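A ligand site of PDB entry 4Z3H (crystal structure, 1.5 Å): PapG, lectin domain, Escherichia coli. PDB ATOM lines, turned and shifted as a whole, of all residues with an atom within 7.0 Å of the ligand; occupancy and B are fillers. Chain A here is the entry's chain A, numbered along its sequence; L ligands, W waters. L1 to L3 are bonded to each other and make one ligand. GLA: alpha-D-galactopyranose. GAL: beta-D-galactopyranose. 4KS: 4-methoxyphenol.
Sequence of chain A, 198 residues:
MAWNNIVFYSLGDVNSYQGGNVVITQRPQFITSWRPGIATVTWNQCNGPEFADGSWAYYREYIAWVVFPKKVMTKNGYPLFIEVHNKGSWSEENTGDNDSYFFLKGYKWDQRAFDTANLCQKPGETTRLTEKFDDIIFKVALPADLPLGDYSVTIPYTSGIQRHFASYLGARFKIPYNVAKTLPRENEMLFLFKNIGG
Merely in contact with the ligand: Ser 91 (3.8 Å), Leu 104 (3.8 Å), Lys 105 (3.6 Å), Trp 109 (3.4 Å) and Arg 172 (3.5 Å).
Hydrophobic or aromatic side chains that line the ligand: Leu 104 and Trp 109.
Of the 20 residues printed, 9 come within 4 Å of the ligand.
Water W3 lies within hydrogen-bond range of O6 of GLA L1 (2.6 Å) and NZ of Lys 105 (2.9 Å).
Water W2 lies within hydrogen-bond range of O6 of GAL L2 (2.7 Å), O of Lys 108 (2.9 Å), O of Tyr 62 (3.0 Å) and N of Tyr 107 (3.2 Å).
Water W6 bridges O2 of GLA L1 and OE1 of Glu 61.
The side-chain carboxylate (OE2) of Glu 61 is in hydrogen-bond range of the backbone NH (N) of Phe 173, 3.0 Å away.
The side-chain carboxylate of Glu 93 lies within salt-bridge range of the side-chain amino group of Lys 174.
The side-chain hydroxyl (OG) of Ser 91 lies within hydrogen-bond range of the side-chain carboxylate (OE2) of Glu 93, 2.7 Å away.
The side-chain carboxylate (OE1) of Glu 93 lies within hydrogen-bond range of the side-chain hydroxyl (OH) of Tyr 177, at 2.5 Å.
OD1 of Asp 110 is in salt-bridge range of NH1 of Arg 172 (2.8 Å).
O of Ser 89 is in hydrogen-bond range of NZ of Lys 105 (2.8 Å).
The backbone carbonyl oxygen of Lys 105 is in hydrogen-bond range of the backbone NH of Ala 64, 2.8 Å away.
The backbone NH of Leu 104 sits at hydrogen-bond distance from the backbone carbonyl oxygen of Ser 91 (2.9 Å).
O6 of GAL L2 is in hydrogen-bond range of OE1 of Glu 61 (2.6 Å).
The side-chain carboxylate (OE2) of Glu 93 lies within hydrogen-bond range of an oxygen (O4) of GLA L1 (2.7 Å).
N of Gly 106 lies within hydrogen-bond range of O6 of GLA L1 (2.8 Å).
O3 of GAL L2 lies within hydrogen-bond range of O of Gly 106 (2.9 Å).
O3 of GLA L1 sits at hydrogen-bond distance from NZ of Lys 174 (2.9 Å).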
ATOM      1  N   GLU A  61     -20.882 -21.463   5.817  1.00  0.00           N
ATOM      2  CA  GLU A  61     -19.937 -21.868   6.875  1.00  0.00           C
ATOM      3  C   GLU A  61     -20.475 -23.172   7.451  1.00  0.00           C
ATOM      4  O   GLU A  61     -21.605 -23.183   7.975  1.00  0.00           O
ATOM      5  CB  GLU A  61     -19.800 -20.806   7.980  1.00  0.00           C
ATOM      6  CG  GLU A  61     -18.842 -21.239   9.095  1.00  0.00           C
ATOM      7  CD  GLU A  61     -18.874 -20.368  10.341  1.00  0.00           C
ATOM      8  OE1 GLU A  61     -17.807 -20.209  10.973  1.00  0.00           O
ATOM      9  OE2 GLU A  61     -19.964 -19.885  10.705  1.00  0.00           O
ATOM     10  N   TYR A  62     -19.701 -24.285   7.346  1.00  0.00           N
ATOM     11  CA  TYR A  62     -20.164 -25.576   7.865  1.00  0.00           C
ATOM     12  C   TYR A  62     -19.222 -26.067   8.939  1.00  0.00           C
ATOM     13  O   TYR A  62     -17.989 -25.987   8.762  1.00  0.00           O
ATOM     14  CB  TYR A  62     -20.186 -26.639   6.745  1.00  0.00           C
ATOM     15  CG  TYR A  62     -21.107 -26.411   5.558  1.00  0.00           C
ATOM     16  CD1 TYR A  62     -22.130 -25.461   5.600  1.00  0.00           C
ATOM     17  CD2 TYR A  62     -20.960 -27.160   4.385  1.00  0.00           C
ATOM     18  CE1 TYR A  62     -22.975 -25.247   4.500  1.00  0.00           C
ATOM     19  CE2 TYR A  62     -21.818 -26.970   3.294  1.00  0.00           C
ATOM     20  CZ  TYR A  62     -22.820 -26.015   3.358  1.00  0.00           C
ATOM     21  OH  TYR A  62     -23.642 -25.801   2.291  1.00  0.00           O
ATOM     22  N   ILE A  63     -19.766 -26.581  10.032  1.00  0.00           N
ATOM     23  CA  ILE A  63     -18.953 -27.087  11.150  1.00  0.00           C
ATOM     24  C   ILE A  63     -19.534 -28.409  11.643  1.00  0.00           C
ATOM     25  O   ILE A  63     -20.727 -28.446  11.957  1.00  0.00           O
ATOM     26  CB  ILE A  63     -18.913 -26.093  12.334  1.00  0.00           C
ATOM     27  CG1 ILE A  63     -18.458 -24.695  11.877  1.00  0.00           C
ATOM     28  CG2 ILE A  63     -18.093 -26.670  13.516  1.00  0.00           C
ATOM     29  CD1 ILE A  63     -18.424 -23.663  13.022  1.00  0.00           C
ATOM     30  N   ALA A  64     -18.757 -29.478  11.607  1.00  0.00           N
ATOM     31  CA  ALA A  64     -19.234 -30.751  12.150  1.00  0.00           C
ATOM     32  C   ALA A  64     -19.034 -30.776  13.659  1.00  0.00           C
ATOM     33  O   ALA A  64     -18.049 -30.227  14.170  1.00  0.00           O
ATOM     34  CB  ALA A  64     -18.430 -31.892  11.556  1.00  0.00           C
ATOM     35  N   SER A  89      -8.114 -35.455  13.918  1.00  0.00           N
ATOM     36  CA  SER A  89      -7.995 -34.040  13.534  1.00  0.00           C
ATOM     37  C   SER A  89      -9.036 -33.153  14.237  1.00  0.00           C
ATOM     38  O   SER A  89      -9.049 -31.939  14.021  1.00  0.00           O
ATOM     39  CB  SER A  89      -8.155 -33.909  12.025  1.00  0.00           C
ATOM     40  OG  SER A  89      -9.459 -34.312  11.651  1.00  0.00           O
ATOM     41  N   TRP A  90      -9.909 -33.730  15.067  1.00  0.00           N
ATOM     42  CA  TRP A  90     -10.955 -32.944  15.705  1.00  0.00           C
ATOM     43  C   TRP A  90     -10.421 -31.884  16.647  1.00  0.00           C
ATOM     44  O   TRP A  90      -9.403 -32.090  17.326  1.00  0.00           O
ATOM     45  CB  TRP A  90     -11.888 -33.871  16.499  1.00  0.00           C
ATOM     46  CG  TRP A  90     -12.761 -34.773  15.635  1.00  0.00           C
ATOM     47  CD1 TRP A  90     -12.545 -36.097  15.352  1.00  0.00           C
ATOM     48  CD2 TRP A  90     -14.055 -34.455  15.088  1.00  0.00           C
ATOM     49  NE1 TRP A  90     -13.596 -36.602  14.610  1.00  0.00           N
ATOM     50  CE2 TRP A  90     -14.509 -35.602  14.397  1.00  0.00           C
ATOM     51  CE3 TRP A  90     -14.844 -33.297  15.074  1.00  0.00           C
ATOM     52  CZ2 TRP A  90     -15.754 -35.633  13.754  1.00  0.00           C
ATOM     53  CZ3 TRP A  90     -16.063 -33.310  14.425  1.00  0.00           C
ATOM     54  CH2 TRP A  90     -16.511 -34.471  13.751  1.00  0.00           C
ATOM     55  N   SER A  91     -11.150 -30.752  16.734  1.00  0.00           N
ATOM     56  CA  SER A  91     -10.818 -29.685  17.673  1.00  0.00           C
ATOM     57  C   SER A  91     -11.573 -29.976  18.962  1.00  0.00           C
ATOM     58  O   SER A  91     -12.809 -29.925  18.973  1.00  0.00           O
ATOM     59  CB  SER A  91     -11.233 -28.335  17.081  1.00  0.00           C
ATOM     60  OG  SER A  91     -10.936 -27.267  17.973  1.00  0.00           O
ATOM     61  N   GLU A  93     -12.861 -28.851  22.347  1.00  0.00           N
ATOM     62  CA  GLU A  93     -13.133 -27.513  22.883  1.00  0.00           C
ATOM     63  C   GLU A  93     -13.932 -27.502  24.159  1.00  0.00           C
ATOM     64  O   GLU A  93     -14.506 -28.543  24.552  1.00  0.00           O
ATOM     65  CB  GLU A  93     -13.883 -26.694  21.818  1.00  0.00           C
ATOM     66  CG  GLU A  93     -13.078 -26.557  20.532  1.00  0.00           C
ATOM     67  CD  GLU A  93     -13.681 -25.711  19.441  1.00  0.00           C
ATOM     68  OE1 GLU A  93     -14.647 -24.977  19.724  1.00  0.00           O
ATOM     69  OE2 GLU A  93     -13.121 -25.720  18.327  1.00  0.00           O
ATOM     70  N   LEU A 104     -15.143 -30.428  17.386  1.00  0.00           N
ATOM     71  CA  LEU A 104     -15.632 -29.652  16.254  1.00  0.00           C
ATOM     72  C   LEU A 104     -14.703 -29.782  15.071  1.00  0.00           C
ATOM     73  O   LEU A 104     -13.487 -29.953  15.243  1.00  0.00           O
ATOM     74  CB  LEU A 104     -15.713 -28.161  16.646  1.00  0.00           C
ATOM     75  CG  LEU A 104     -16.923 -27.766  17.491  1.00  0.00           C
ATOM     76  CD1 LEU A 104     -16.702 -28.159  18.987  1.00  0.00           C
ATOM     77  CD2 LEU A 104     -17.073 -26.260  17.489  1.00  0.00           C
ATOM     78  N   LYS A 105     -15.254 -29.667  13.854  1.00  0.00           N
ATOM     79  CA  LYS A 105     -14.400 -29.558  12.671  1.00  0.00           C
ATOM     80  C   LYS A 105     -15.033 -28.582  11.707  1.00  0.00           C
ATOM     81  O   LYS A 105     -16.030 -28.906  11.042  1.00  0.00           O
ATOM     82  CB  LYS A 105     -14.121 -30.919  12.004  1.00  0.00           C
ATOM     83  CG  LYS A 105     -13.251 -30.790  10.726  1.00  0.00           C
ATOM     84  CD  LYS A 105     -11.886 -30.058  10.937  1.00  0.00           C
ATOM     85  CE  LYS A 105     -11.059 -30.644  12.046  1.00  0.00           C
ATOM     86  NZ  LYS A 105      -9.659 -30.065  12.097  1.00  0.00           N
ATOM     87  N   GLY A 106     -14.459 -27.383  11.661  1.00  0.00           N
ATOM     88  CA  GLY A 106     -14.964 -26.322  10.786  1.00  0.00           C
ATOM     89  C   GLY A 106     -14.203 -26.450   9.483  1.00  0.00           C
ATOM     90  O   GLY A 106     -13.002 -26.197   9.458  1.00  0.00           O
ATOM     91  N   TYR A 107     -14.891 -26.922   8.429  1.00  0.00           N
ATOM     92  CA  TYR A 107     -14.246 -27.276   7.154  1.00  0.00           C
ATOM     93  C   TYR A 107     -14.641 -26.452   5.952  1.00  0.00           C
ATOM     94  O   TYR A 107     -14.138 -26.681   4.833  1.00  0.00           O
ATOM     95  CB  TYR A 107     -14.510 -28.782   6.871  1.00  0.00           C
ATOM     96  CG  TYR A 107     -15.968 -29.116   6.667  1.00  0.00           C
ATOM     97  CD1 TYR A 107     -16.829 -29.297   7.749  1.00  0.00           C
ATOM     98  CD2 TYR A 107     -16.514 -29.235   5.389  1.00  0.00           C
ATOM     99  CE1 TYR A 107     -18.178 -29.607   7.562  1.00  0.00           C
ATOM    100  CE2 TYR A 107     -17.846 -29.568   5.191  1.00  0.00           C
ATOM    101  CZ  TYR A 107     -18.682 -29.756   6.289  1.00  0.00           C
ATOM    102  OH  TYR A 107     -20.001 -30.095   6.094  1.00  0.00           O
ATOM    103  N   LYS A 108     -15.543 -25.474   6.164  1.00  0.00           N
ATOM    104  CA  LYS A 108     -15.967 -24.591   5.088  1.00  0.00           C
ATOM    105  C   LYS A 108     -16.349 -23.253   5.684  1.00  0.00           C
ATOM    106  O   LYS A 108     -17.087 -23.216   6.667  1.00  0.00           O
ATOM    107  CB  LYS A 108     -17.204 -25.165   4.366  1.00  0.00           C
ATOM    108  CG  LYS A 108     -17.629 -24.353   3.135  1.00  0.00           C
ATOM    109  CD  LYS A 108     -18.860 -24.969   2.465  1.00  0.00           C
ATOM    110  CE  LYS A 108     -18.606 -26.316   1.801  1.00  0.00           C
ATOM    111  NZ  LYS A 108     -17.545 -26.225   0.768  1.00  0.00           N
ATOM    112  N   TRP A 109     -15.837 -22.169   5.104  1.00  0.00           N
ATOM    113  CA  TRP A 109     -16.193 -20.841   5.607  1.00  0.00           C
ATOM    114  C   TRP A 109     -16.057 -19.834   4.518  1.00  0.00           C
ATOM    115  O   TRP A 109     -15.260 -20.044   3.592  1.00  0.00           O
ATOM    116  CB  TRP A 109     -15.289 -20.450   6.796  1.00  0.00           C
ATOM    117  CG  TRP A 109     -13.811 -20.479   6.494  1.00  0.00           C
ATOM    118  CD1 TRP A 109     -13.044 -19.423   6.083  1.00  0.00           C
ATOM    119  CD2 TRP A 109     -12.930 -21.620   6.549  1.00  0.00           C
ATOM    120  NE1 TRP A 109     -11.744 -19.828   5.881  1.00  0.00           N
ATOM    121  CE2 TRP A 109     -11.642 -21.169   6.179  1.00  0.00           C
ATOM    122  CE3 TRP A 109     -13.103 -22.971   6.913  1.00  0.00           C
ATOM    123  CZ2 TRP A 109     -10.534 -22.022   6.131  1.00  0.00           C
ATOM    124  CZ3 TRP A 109     -12.008 -23.818   6.862  1.00  0.00           C
ATOM    125  CH2 TRP A 109     -10.738 -23.349   6.472  1.00  0.00           C
ATOM    126  N   ASP A 110     -16.821 -18.726   4.603  1.00  0.00           N
ATOM    127  CA  ASP A 110     -16.691 -17.595   3.666  1.00  0.00           C
ATOM    128  C   ASP A 110     -16.853 -18.006   2.209  1.00  0.00           C
ATOM    129  O   ASP A 110     -16.327 -17.321   1.303  1.00  0.00           O
ATOM    130  CB  ASP A 110     -15.308 -16.926   3.851  1.00  0.00           C
ATOM    131  CG  ASP A 110     -15.165 -16.251   5.192  1.00  0.00           C
ATOM    132  OD1 ASP A 110     -16.186 -15.948   5.814  1.00  0.00           O
ATOM    133  OD2 ASP A 110     -14.005 -16.096   5.666  1.00  0.00           O
ATOM    134  N   ALA A 171     -18.973 -14.086   7.680  1.00  0.00           N
ATOM    135  CA  ALA A 171     -19.941 -14.512   8.690  1.00  0.00           C
ATOM    136  C   ALA A 171     -19.430 -15.668   9.530  1.00  0.00           C
ATOM    137  O   ALA A 171     -18.855 -16.635   8.990  1.00  0.00           O
ATOM    138  CB  ALA A 171     -21.256 -14.892   8.021  1.00  0.00           C
ATOM    139  N   ARG A 172     -19.637 -15.588  10.851  1.00  0.00           N
ATOM    140  CA  ARG A 172     -19.187 -16.635  11.749  1.00  0.00           C
ATOM    141  C   ARG A 172     -20.263 -16.880  12.783  1.00  0.00           C
ATOM    142  O   ARG A 172     -20.805 -15.938  13.369  1.00  0.00           O
ATOM    143  CB  ARG A 172     -17.920 -16.198  12.554  1.00  0.00           C
ATOM    144  CG  ARG A 172     -16.670 -15.916  11.720  1.00  0.00           C
ATOM    145  CD  ARG A 172     -15.998 -17.200  11.270  1.00  0.00           C
ATOM    146  NE  ARG A 172     -14.822 -16.909  10.461  1.00  0.00           N
ATOM    147  CZ  ARG A 172     -14.851 -16.637   9.160  1.00  0.00           C
ATOM    148  NH1 ARG A 172     -16.002 -16.711   8.475  1.00  0.00           N
ATOM    149  NH2 ARG A 172     -13.735 -16.313   8.520  1.00  0.00           N
ATOM    150  N   PHE A 173     -20.545 -18.150  13.029  1.00  0.00           N
ATOM    151  CA  PHE A 173     -21.474 -18.523  14.073  1.00  0.00           C
ATOM    152  C   PHE A 173     -21.128 -19.929  14.521  1.00  0.00           C
ATOM    153  O   PHE A 173     -20.982 -20.823  13.664  1.00  0.00           O
ATOM    154  CB  PHE A 173     -22.943 -18.502  13.592  1.00  0.00           C
ATOM    155  CG  PHE A 173     -23.930 -18.841  14.704  1.00  0.00           C
ATOM    156  CD1 PHE A 173     -24.258 -20.152  14.999  1.00  0.00           C
ATOM    157  CD2 PHE A 173     -24.509 -17.836  15.457  1.00  0.00           C
ATOM    158  CE1 PHE A 173     -25.168 -20.457  16.025  1.00  0.00           C
ATOM    159  CE2 PHE A 173     -25.398 -18.140  16.494  1.00  0.00           C
ATOM    160  CZ  PHE A 173     -25.719 -19.451  16.757  1.00  0.00           C
ATOM    161  N   LYS A 174     -21.035 -20.132  15.850  1.00  0.00           N
ATOM    162  CA  LYS A 174     -20.822 -21.453  16.408  1.00  0.00           C
ATOM    163  C   LYS A 174     -21.968 -21.656  17.387  1.00  0.00           C
ATOM    164  O   LYS A 174     -22.247 -20.782  18.224  1.00  0.00           O
ATOM    165  CB  LYS A 174     -19.448 -21.487  17.086  1.00  0.00           C
ATOM    166  CG  LYS A 174     -19.087 -22.839  17.665  1.00  0.00           C
ATOM    167  CD  LYS A 174     -17.775 -22.777  18.473  1.00  0.00           C
ATOM    168  CE  LYS A 174     -16.573 -22.591  17.592  1.00  0.00           C
ATOM    169  NZ  LYS A 174     -15.316 -22.523  18.383  1.00  0.00           N
ATOM    170  N   TYR A 177     -21.916 -23.652  23.293  1.00  0.00           N
ATOM    171  CA  TYR A 177     -21.669 -24.962  23.924  1.00  0.00           C
ATOM    172  C   TYR A 177     -22.838 -25.383  24.822  1.00  0.00           C
ATOM    173  O   TYR A 177     -23.177 -26.569  24.843  1.00  0.00           O
ATOM    174  CB  TYR A 177     -20.352 -24.984  24.725  1.00  0.00           C
ATOM    175  CG  TYR A 177     -19.120 -24.646  23.899  1.00  0.00           C
ATOM    176  CD1 TYR A 177     -18.696 -25.496  22.873  1.00  0.00           C
ATOM    177  CD2 TYR A 177     -18.370 -23.514  24.175  1.00  0.00           C
ATOM    178  CE1 TYR A 177     -17.567 -25.180  22.106  1.00  0.00           C
ATOM    179  CE2 TYR A 177     -17.208 -23.223  23.453  1.00  0.00           C
ATOM    180  CZ  TYR A 177     -16.832 -24.034  22.397  1.00  0.00           C
ATOM    181  OH  TYR A 177     -15.683 -23.730  21.691  1.00  0.00           O
HETATM  182  C1  GLA L   1     -14.223 -22.941  13.005  1.00  0.00           C
HETATM  183  C2  GLA L   1     -14.435 -22.182  14.323  1.00  0.00           C
HETATM  184  C3  GLA L   1     -13.177 -22.329  15.198  1.00  0.00           C
HETATM  185  C4  GLA L   1     -12.946 -23.797  15.548  1.00  0.00           C
HETATM  186  C5  GLA L   1     -12.774 -24.567  14.211  1.00  0.00           C
HETATM  187  C6  GLA L   1     -12.795 -26.066  14.462  1.00  0.00           C
HETATM  188  O2  GLA L   1     -14.669 -20.785  14.048  1.00  0.00           O
HETATM  189  O3  GLA L   1     -13.395 -21.602  16.452  1.00  0.00           O
HETATM  190  O4  GLA L   1     -14.111 -24.277  16.264  1.00  0.00           O
HETATM  191  O5  GLA L   1     -13.952 -24.306  13.345  1.00  0.00           O
HETATM  192  O6  GLA L   1     -12.281 -26.772  13.301  1.00  0.00           O
HETATM  193  C1  GAL L   2     -10.890 -20.886  10.107  1.00  0.00           C
HETATM  194  C2  GAL L   2     -10.560 -22.207  10.802  1.00  0.00           C
HETATM  195  C3  GAL L   2     -11.675 -23.201  10.456  1.00  0.00           C
HETATM  196  C4  GAL L   2     -13.047 -22.643  10.872  1.00  0.00           C
HETATM  197  C5  GAL L   2     -13.214 -21.287  10.126  1.00  0.00           C
HETATM  198  C6  GAL L   2     -14.497 -20.554  10.502  1.00  0.00           C
HETATM  199  O2  GAL L   2      -9.307 -22.738  10.336  1.00  0.00           O
HETATM  200  O3  GAL L   2     -11.447 -24.440  11.132  1.00  0.00           O
HETATM  201  O4  GAL L   2     -13.063 -22.403  12.318  1.00  0.00           O
HETATM  202  O5  GAL L   2     -12.166 -20.386  10.574  1.00  0.00           O
HETATM  203  O6  GAL L   2     -15.620 -21.425  10.277  1.00  0.00           O
HETATM  204  C4  4KS L   3      -9.776 -18.800   9.809  1.00  0.00           C
HETATM  205  C5  4KS L   3     -10.644 -18.364   8.785  1.00  0.00           C
HETATM  206  C6  4KS L   3     -10.405 -17.131   8.137  1.00  0.00           C
HETATM  207  O1  4KS L   3      -9.927 -19.958  10.528  1.00  0.00           O
HETATM  208  C3  4KS L   3      -8.673 -18.024  10.195  1.00  0.00           C
HETATM  209  C2  4KS L   3      -8.453 -16.801   9.539  1.00  0.00           C
HETATM  210  C1  4KS L   3      -9.299 -16.363   8.526  1.00  0.00           C
HETATM  211  O   4KS L   3      -8.998 -15.139   7.962  1.00  0.00           O
HETATM  212  C   4KS L   3      -9.872 -14.652   6.926  1.00  0.00           C
HETATM  213  O   HOH W   1      -8.675 -24.884   8.916  1.00  0.00           O
HETATM  214  O   HOH W   2     -15.824 -23.931   9.201  1.00  0.00           O
HETATM  215  O   HOH W   3      -9.712 -27.367  13.086  1.00  0.00           O
HETATM  216  O   HOH W   4      -9.080 -24.825  12.771  1.00  0.00           O
HETATM  217  O   HOH W   5     -13.142 -18.884  16.412  1.00  0.00           O
HETATM  218  O   HOH W   6     -17.259 -19.792  13.759  1.00  0.00           O
